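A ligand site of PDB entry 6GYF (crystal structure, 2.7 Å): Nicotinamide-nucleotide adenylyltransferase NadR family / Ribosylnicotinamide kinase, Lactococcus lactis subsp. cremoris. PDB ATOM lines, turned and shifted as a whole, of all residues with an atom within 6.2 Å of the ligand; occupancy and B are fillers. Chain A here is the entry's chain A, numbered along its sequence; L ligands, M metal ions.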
ATOM      1  N   GLY A  60      25.523 -26.980 -18.959  1.00  0.00           N
ATOM      2  CA  GLY A  60      26.047 -26.066 -17.964  1.00  0.00           C
ATOM      3  C   GLY A  60      25.066 -25.632 -16.890  1.00  0.00           C
ATOM      4  O   GLY A  60      25.281 -24.576 -16.280  1.00  0.00           O
ATOM      5  N   LEU A  61      24.019 -26.406 -16.623  1.00  0.00           N
ATOM      6  CA  LEU A  61      23.077 -26.143 -15.540  1.00  0.00           C
ATOM      7  C   LEU A  61      22.991 -27.371 -14.661  1.00  0.00           C
ATOM      8  O   LEU A  61      21.983 -28.096 -14.652  1.00  0.00           O
ATOM      9  CB  LEU A  61      21.685 -25.761 -16.067  1.00  0.00           C
ATOM     10  CG  LEU A  61      21.470 -24.438 -16.799  1.00  0.00           C
ATOM     11  CD1 LEU A  61      20.000 -24.295 -17.054  1.00  0.00           C
ATOM     12  CD2 LEU A  61      21.948 -23.280 -15.964  1.00  0.00           C
ATOM     13  N   LYS A  65      23.446 -25.362  -9.636  1.00  0.00           N
ATOM     14  CA  LYS A  65      23.154 -24.084 -10.284  1.00  0.00           C
ATOM     15  C   LYS A  65      21.652 -23.921 -10.535  1.00  0.00           C
ATOM     16  O   LYS A  65      21.109 -22.835 -10.331  1.00  0.00           O
ATOM     17  CB  LYS A  65      23.945 -23.961 -11.586  1.00  0.00           C
ATOM     18  CG  LYS A  65      23.900 -22.571 -12.225  1.00  0.00           C
ATOM     19  CD  LYS A  65      24.778 -22.473 -13.483  1.00  0.00           C
ATOM     20  CE  LYS A  65      26.074 -21.673 -13.241  1.00  0.00           C
ATOM     21  NZ  LYS A  65      27.207 -22.022 -14.180  1.00  0.00           N
ATOM     22  N   TYR A  69      19.314 -20.830  -8.972  1.00  0.00           N
ATOM     23  CA  TYR A  69      18.502 -20.005  -9.854  1.00  0.00           C
ATOM     24  C   TYR A  69      17.024 -20.061  -9.471  1.00  0.00           C
ATOM     25  O   TYR A  69      16.303 -19.056  -9.557  1.00  0.00           O
ATOM     26  CB  TYR A  69      18.674 -20.454 -11.304  1.00  0.00           C
ATOM     27  CG  TYR A  69      19.956 -20.068 -12.006  1.00  0.00           C
ATOM     28  CD1 TYR A  69      21.008 -19.437 -11.351  1.00  0.00           C
ATOM     29  CD2 TYR A  69      20.086 -20.302 -13.367  1.00  0.00           C
ATOM     30  CE1 TYR A  69      22.176 -19.092 -12.034  1.00  0.00           C
ATOM     31  CE2 TYR A  69      21.237 -19.960 -14.064  1.00  0.00           C
ATOM     32  CZ  TYR A  69      22.272 -19.354 -13.410  1.00  0.00           C
ATOM     33  OH  TYR A  69      23.408 -19.029 -14.156  1.00  0.00           O
ATOM     34  N   ARG A 177      20.473 -15.334 -17.943  1.00  0.00           N
ATOM     35  CA  ARG A 177      21.877 -15.044 -17.679  1.00  0.00           C
ATOM     36  C   ARG A 177      22.786 -16.033 -18.397  1.00  0.00           C
ATOM     37  O   ARG A 177      23.784 -15.634 -19.008  1.00  0.00           O
ATOM     38  CB  ARG A 177      22.079 -15.049 -16.150  1.00  0.00           C
ATOM     39  CG  ARG A 177      23.531 -15.142 -15.623  1.00  0.00           C
ATOM     40  CD  ARG A 177      23.608 -15.209 -14.042  1.00  0.00           C
ATOM     41  NE  ARG A 177      24.529 -16.266 -13.532  1.00  0.00           N
ATOM     42  CZ  ARG A 177      24.964 -16.372 -12.272  1.00  0.00           C
ATOM     43  NH1 ARG A 177      24.595 -15.500 -11.341  1.00  0.00           N
ATOM     44  NH2 ARG A 177      25.775 -17.375 -11.927  1.00  0.00           N
ATOM     45  N   HIS A 178      22.383 -17.314 -18.413  1.00  0.00           N
ATOM     46  CA  HIS A 178      23.179 -18.438 -18.912  1.00  0.00           C
ATOM     47  C   HIS A 178      23.054 -18.713 -20.409  1.00  0.00           C
ATOM     48  O   HIS A 178      23.984 -19.247 -21.001  1.00  0.00           O
ATOM     49  CB  HIS A 178      22.765 -19.703 -18.161  1.00  0.00           C
ATOM     50  CG  HIS A 178      23.468 -20.943 -18.634  1.00  0.00           C
ATOM     51  ND1 HIS A 178      24.750 -21.274 -18.247  1.00  0.00           N
ATOM     52  CD2 HIS A 178      23.048 -21.945 -19.449  1.00  0.00           C
ATOM     53  CE1 HIS A 178      25.096 -22.414 -18.803  1.00  0.00           C
ATOM     54  NE2 HIS A 178      24.091 -22.831 -19.546  1.00  0.00           N
ATOM     55  N   VAL A 182      26.963 -14.169 -26.933  1.00  0.00           N
ATOM     56  CA  VAL A 182      27.851 -13.070 -26.605  1.00  0.00           C
ATOM     57  C   VAL A 182      28.757 -12.799 -27.798  1.00  0.00           C
ATOM     58  O   VAL A 182      29.491 -13.675 -28.241  1.00  0.00           O
ATOM     59  CB  VAL A 182      28.698 -13.369 -25.356  1.00  0.00           C
ATOM     60  CG1 VAL A 182      29.757 -12.298 -25.179  1.00  0.00           C
ATOM     61  CG2 VAL A 182      27.833 -13.502 -24.098  1.00  0.00           C
ATOM     62  N   THR A 184      31.845 -10.230 -28.835  1.00  0.00           N
ATOM     63  CA  THR A 184      32.810  -9.302 -28.276  1.00  0.00           C
ATOM     64  C   THR A 184      33.606  -8.667 -29.411  1.00  0.00           C
ATOM     65  O   THR A 184      34.097  -9.379 -30.288  1.00  0.00           O
ATOM     66  CB  THR A 184      33.754 -10.001 -27.286  1.00  0.00           C
ATOM     67  OG1 THR A 184      33.001 -10.496 -26.180  1.00  0.00           O
ATOM     68  CG2 THR A 184      34.838  -9.059 -26.816  1.00  0.00           C
ATOM     69  N   GLN A 239      35.583  -3.587 -16.443  1.00  0.00           N
ATOM     70  CA  GLN A 239      35.060  -3.954 -17.749  1.00  0.00           C
ATOM     71  C   GLN A 239      34.207  -5.222 -17.666  1.00  0.00           C
ATOM     72  O   GLN A 239      33.146  -5.318 -18.299  1.00  0.00           O
ATOM     73  CB  GLN A 239      36.211  -4.144 -18.748  1.00  0.00           C
ATOM     74  CG  GLN A 239      35.811  -4.402 -20.216  1.00  0.00           C
ATOM     75  CD  GLN A 239      35.186  -3.210 -20.916  1.00  0.00           C
ATOM     76  OE1 GLN A 239      35.877  -2.253 -21.266  1.00  0.00           O
ATOM     77  NE2 GLN A 239      33.879  -3.256 -21.145  1.00  0.00           N
ATOM     78  N   TYR A 240      34.641  -6.187 -16.847  1.00  0.00           N
ATOM     79  CA  TYR A 240      33.867  -7.405 -16.688  1.00  0.00           C
ATOM     80  C   TYR A 240      32.501  -7.116 -16.077  1.00  0.00           C
ATOM     81  O   TYR A 240      31.481  -7.628 -16.546  1.00  0.00           O
ATOM     82  CB  TYR A 240      34.650  -8.416 -15.853  1.00  0.00           C
ATOM     83  CG  TYR A 240      33.924  -9.699 -15.664  1.00  0.00           C
ATOM     84  CD1 TYR A 240      33.006  -9.844 -14.631  1.00  0.00           C
ATOM     85  CD2 TYR A 240      34.155 -10.768 -16.503  1.00  0.00           C
ATOM     86  CE1 TYR A 240      32.339 -11.033 -14.436  1.00  0.00           C
ATOM     87  CE2 TYR A 240      33.479 -11.972 -16.323  1.00  0.00           C
ATOM     88  CZ  TYR A 240      32.575 -12.097 -15.282  1.00  0.00           C
ATOM     89  OH  TYR A 240      31.890 -13.282 -15.096  1.00  0.00           O
ATOM     90  N   ASP A 241      32.468  -6.320 -15.007  1.00  0.00           N
ATOM     91  CA  ASP A 241      31.184  -5.950 -14.423  1.00  0.00           C
ATOM     92  C   ASP A 241      30.284  -5.311 -15.465  1.00  0.00           C
ATOM     93  O   ASP A 241      29.098  -5.656 -15.575  1.00  0.00           O
ATOM     94  CB  ASP A 241      31.391  -5.005 -13.238  1.00  0.00           C
ATOM     95  CG  ASP A 241      32.052  -5.691 -12.046  1.00  0.00           C
ATOM     96  OD1 ASP A 241      32.188  -6.946 -12.088  1.00  0.00           O
ATOM     97  OD2 ASP A 241      32.432  -4.977 -11.064  1.00  0.00           O
ATOM     98  N   ASN A 243      30.328  -5.595 -18.799  1.00  0.00           N
ATOM     99  CA  ASN A 243      29.873  -6.575 -19.762  1.00  0.00           C
ATOM    100  C   ASN A 243      28.853  -7.521 -19.118  1.00  0.00           C
ATOM    101  O   ASN A 243      27.807  -7.812 -19.706  1.00  0.00           O
ATOM    102  CB  ASN A 243      31.092  -7.304 -20.327  1.00  0.00           C
ATOM    103  CG  ASN A 243      31.961  -6.365 -21.136  1.00  0.00           C
ATOM    104  OD1 ASN A 243      31.508  -5.300 -21.539  1.00  0.00           O
ATOM    105  ND2 ASN A 243      33.206  -6.732 -21.341  1.00  0.00           N
ATOM    106  N   SER A 244      29.145  -7.982 -17.890  1.00  0.00           N
ATOM    107  CA  SER A 244      28.190  -8.784 -17.132  1.00  0.00           C
ATOM    108  C   SER A 244      26.872  -8.054 -16.942  1.00  0.00           C
ATOM    109  O   SER A 244      25.800  -8.686 -16.915  1.00  0.00           O
ATOM    110  CB  SER A 244      28.779  -9.168 -15.786  1.00  0.00           C
ATOM    111  OG  SER A 244      27.903 -10.011 -15.070  1.00  0.00           O
ATOM    112  N   ARG A 245      26.909  -6.736 -16.820  1.00  0.00           N
ATOM    113  CA  ARG A 245      25.661  -6.014 -16.614  1.00  0.00           C
ATOM    114  C   ARG A 245      24.803  -6.074 -17.862  1.00  0.00           C
ATOM    115  O   ARG A 245      23.573  -6.227 -17.774  1.00  0.00           O
ATOM    116  CB  ARG A 245      25.952  -4.572 -16.190  1.00  0.00           C
ATOM    117  CG  ARG A 245      24.819  -3.831 -15.489  1.00  0.00           C
ATOM    118  CD  ARG A 245      25.327  -2.555 -14.832  1.00  0.00           C
ATOM    119  NE  ARG A 245      26.376  -2.862 -13.852  1.00  0.00           N
ATOM    120  CZ  ARG A 245      27.663  -2.547 -13.985  1.00  0.00           C
ATOM    121  NH1 ARG A 245      28.540  -2.873 -13.041  1.00  0.00           N
ATOM    122  NH2 ARG A 245      28.075  -1.868 -15.064  1.00  0.00           N
ATOM    123  N   VAL A 247      25.087  -8.490 -20.353  1.00  0.00           N
ATOM    124  CA  VAL A 247      24.687  -9.902 -20.498  1.00  0.00           C
ATOM    125  C   VAL A 247      23.405 -10.186 -19.714  1.00  0.00           C
ATOM    126  O   VAL A 247      22.524 -10.906 -20.184  1.00  0.00           O
ATOM    127  CB  VAL A 247      25.841 -10.823 -20.054  1.00  0.00           C
ATOM    128  CG1 VAL A 247      25.411 -12.275 -20.066  1.00  0.00           C
ATOM    129  CG2 VAL A 247      27.045 -10.640 -20.946  1.00  0.00           C
ATOM    130  N   ASN A 248      23.282  -9.607 -18.518  1.00  0.00           N
ATOM    131  CA  ASN A 248      22.146  -9.845 -17.630  1.00  0.00           C
ATOM    132  C   ASN A 248      21.072  -8.755 -17.723  1.00  0.00           C
ATOM    133  O   ASN A 248      20.143  -8.750 -16.903  1.00  0.00           O
ATOM    134  CB  ASN A 248      22.622 -10.010 -16.186  1.00  0.00           C
ATOM    135  CG  ASN A 248      23.560 -11.193 -16.014  1.00  0.00           C
ATOM    136  OD1 ASN A 248      23.591 -12.078 -16.854  1.00  0.00           O
ATOM    137  ND2 ASN A 248      24.335 -11.211 -14.945  1.00  0.00           N
ATOM    138  N   LEU A 258      29.672  -6.784 -26.778  1.00  0.00           N
ATOM    139  CA  LEU A 258      30.569  -6.291 -25.754  1.00  0.00           C
ATOM    140  C   LEU A 258      31.749  -5.590 -26.397  1.00  0.00           C
ATOM    141  O   LEU A 258      32.423  -6.169 -27.266  1.00  0.00           O
ATOM    142  CB  LEU A 258      31.038  -7.456 -24.865  1.00  0.00           C
ATOM    143  CG  LEU A 258      29.942  -8.269 -24.155  1.00  0.00           C
ATOM    144  CD1 LEU A 258      30.574  -9.305 -23.289  1.00  0.00           C
ATOM    145  CD2 LEU A 258      29.041  -7.370 -23.297  1.00  0.00           C
ATOM    146  N   ASP A 261      37.159  -6.715 -23.667  1.00  0.00           N
ATOM    147  CA  ASP A 261      37.060  -7.662 -22.579  1.00  0.00           C
ATOM    148  C   ASP A 261      38.390  -7.638 -21.835  1.00  0.00           C
ATOM    149  O   ASP A 261      39.174  -6.700 -21.966  1.00  0.00           O
ATOM    150  CB  ASP A 261      36.733  -9.064 -23.139  1.00  0.00           C
ATOM    151  CG  ASP A 261      37.964  -9.714 -23.754  1.00  0.00           C
ATOM    152  OD1 ASP A 261      38.762  -9.021 -24.444  1.00  0.00           O
ATOM    153  OD2 ASP A 261      38.206 -10.912 -23.490  1.00  0.00           O
ATOM    154  N   ASP A 291      36.089 -16.748 -16.831  1.00  0.00           N
ATOM    155  CA  ASP A 291      34.670 -16.503 -16.579  1.00  0.00           C
ATOM    156  C   ASP A 291      33.959 -15.851 -17.759  1.00  0.00           C
ATOM    157  O   ASP A 291      32.764 -15.544 -17.643  1.00  0.00           O
ATOM    158  CB  ASP A 291      34.496 -15.620 -15.338  1.00  0.00           C
ATOM    159  CG  ASP A 291      34.688 -16.376 -14.031  1.00  0.00           C
ATOM    160  OD1 ASP A 291      34.807 -17.625 -14.082  1.00  0.00           O
ATOM    161  OD2 ASP A 291      34.703 -15.733 -12.961  1.00  0.00           O
ATOM    162  N   GLU A 292      34.646 -15.638 -18.892  1.00  0.00           N
ATOM    163  CA  GLU A 292      34.079 -14.925 -20.029  1.00  0.00           C
ATOM    164  C   GLU A 292      33.561 -15.934 -21.042  1.00  0.00           C
ATOM    165  O   GLU A 292      34.333 -16.700 -21.635  1.00  0.00           O
ATOM    166  CB  GLU A 292      35.109 -13.998 -20.679  1.00  0.00           C
ATOM    167  CG  GLU A 292      35.478 -12.756 -19.905  1.00  0.00           C
ATOM    168  CD  GLU A 292      36.328 -11.822 -20.745  1.00  0.00           C
ATOM    169  OE1 GLU A 292      36.523 -12.176 -21.934  1.00  0.00           O
ATOM    170  OE2 GLU A 292      36.817 -10.786 -20.235  1.00  0.00           O
ATOM    171  N   ARG A 293      32.257 -15.926 -21.245  1.00  0.00           N
ATOM    172  CA  ARG A 293      31.614 -16.734 -22.264  1.00  0.00           C
ATOM    173  C   ARG A 293      31.487 -15.874 -23.525  1.00  0.00           C
ATOM    174  O   ARG A 293      30.751 -14.890 -23.525  1.00  0.00           O
ATOM    175  CB  ARG A 293      30.247 -17.207 -21.764  1.00  0.00           C
ATOM    176  CG  ARG A 293      29.779 -18.605 -22.155  1.00  0.00           C
ATOM    177  CD  ARG A 293      28.538 -18.572 -23.092  1.00  0.00           C
ATOM    178  NE  ARG A 293      27.437 -17.625 -22.799  1.00  0.00           N
ATOM    179  CZ  ARG A 293      26.808 -17.453 -21.630  1.00  0.00           C
ATOM    180  NH1 ARG A 293      27.162 -18.126 -20.531  1.00  0.00           N
ATOM    181  NH2 ARG A 293      25.802 -16.582 -21.546  1.00  0.00           N
ATOM    182  N   MET A 294      32.211 -16.246 -24.582  1.00  0.00           N
ATOM    183  CA  MET A 294      32.125 -15.554 -25.859  1.00  0.00           C
ATOM    184  C   MET A 294      31.759 -16.559 -26.944  1.00  0.00           C
ATOM    185  O   MET A 294      32.319 -17.655 -27.003  1.00  0.00           O
ATOM    186  CB  MET A 294      33.450 -14.864 -26.199  1.00  0.00           C
ATOM    187  CG  MET A 294      33.814 -13.788 -25.207  1.00  0.00           C
ATOM    188  SD  MET A 294      35.398 -12.988 -25.517  1.00  0.00           S
ATOM    189  CE  MET A 294      36.553 -14.325 -25.242  1.00  0.00           C
HETATM  190  O1  LIG L   1      28.464 -19.959 -15.283  1.00  0.00           O
HETATM  191  P1  LIG L   1      27.411 -19.368 -16.186  1.00  0.00           P
HETATM  192  O2  LIG L   1      26.014 -19.844 -15.904  1.00  0.00           O
HETATM  193  O3  LIG L   1      27.783 -19.346 -17.652  1.00  0.00           O
HETATM  194  O4  LIG L   1      27.386 -17.809 -15.778  1.00  0.00           O
HETATM  195  C1  LIG L   1      28.172 -16.857 -16.483  1.00  0.00           C
HETATM  196  C2  LIG L   1      28.197 -15.541 -15.716  1.00  0.00           C
HETATM  197  O5  LIG L   1      29.347 -14.780 -16.103  1.00  0.00           O
HETATM  198  C3  LIG L   1      26.962 -14.701 -16.021  1.00  0.00           C
HETATM  199  O6  LIG L   1      26.262 -14.437 -14.797  1.00  0.00           O
HETATM  200  C4  LIG L   1      27.465 -13.443 -16.701  1.00  0.00           C
HETATM  201  O7  LIG L   1      27.061 -12.243 -16.019  1.00  0.00           O
HETATM  202  C5  LIG L   1      28.981 -13.548 -16.722  1.00  0.00           C
HETATM  203  N1  LIG L   1      29.465 -13.524 -18.110  1.00  0.00           N
HETATM  204  C6  LIG L   1      30.306 -12.558 -18.502  1.00  0.00           C
HETATM  205  C7  LIG L   1      30.776 -12.526 -19.811  1.00  0.00           C
HETATM  206  C8  LIG L   1      31.723 -11.450 -20.237  1.00  0.00           C
HETATM  207  O8  LIG L   1      32.206 -11.481 -21.357  1.00  0.00           O
HETATM  208  N2  LIG L   1      32.023 -10.468 -19.380  1.00  0.00           N
HETATM  209  C9  LIG L   1      30.358 -13.481 -20.718  1.00  0.00           C
HETATM  210  C10 LIG L   1      29.477 -14.466 -20.282  1.00  0.00           C
HETATM  211  C11 LIG L   1      29.039 -14.463 -18.969  1.00  0.00           C
HETATM  212 MG    MG M   1      20.948 -14.056 -12.340  1.00  0.00          MG
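Merely in contact with the ligand: Leu 258, Asn 243, Glu 292 and Asp 291.
Hydrophobic or aromatic side chains that line the ligand: His 178, Tyr 240 and Leu 258.
An oxygen (O7) of the ligand is in hydrogen-bond range of the side-chain hydroxyl of Ser 244 (2.6 Å).
NZ of Lys 65 lies within salt-bridge range of O1 of the ligand (2.7 Å).
The guanidinium group (NE) of Arg 177 lies within hydrogen-bond range of an oxygen (O6) of the ligand, 2.8 Å away.
A ring nitrogen (ND1) of His 178 is in hydrogen-bond range of an oxygen (O2) of the ligand (3.0 Å).
The side-chain amide nitrogen of Asn 248 lies within hydrogen-bond range of an oxygen (O7) of the ligand.
OH of Tyr 240 lies within hydrogen-bond range of O5 of the ligand, at 3.1 Å.
NH1 of Arg 293 is in salt-bridge range of O3 of the ligand (3.2 Å).
O2 of the ligand is in hydrogen-bond range of OH of Tyr 69.
The backbone carbonyl oxygen (O) of Arg 177 lies within hydrogen-bond range of the guanidinium group (NH2) of Arg 293 (3.4 Å).
The guanidinium group of Arg 177 is in hydrogen-bond range of the side-chain hydroxyl of Tyr 69, 3.0 Å away.
The guanidinium group of Arg 293 lies within hydrogen-bond range of the backbone carbonyl oxygen of His 178.
NE2 of Gln 239 lies within hydrogen-bond range of OD1 of Asn 243, at 3.2 Å.
The side-chain carboxylate (OE1) of Glu 292 lies close to the side-chain carboxylate (OD2) of Asp 261 (2.6 Å).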
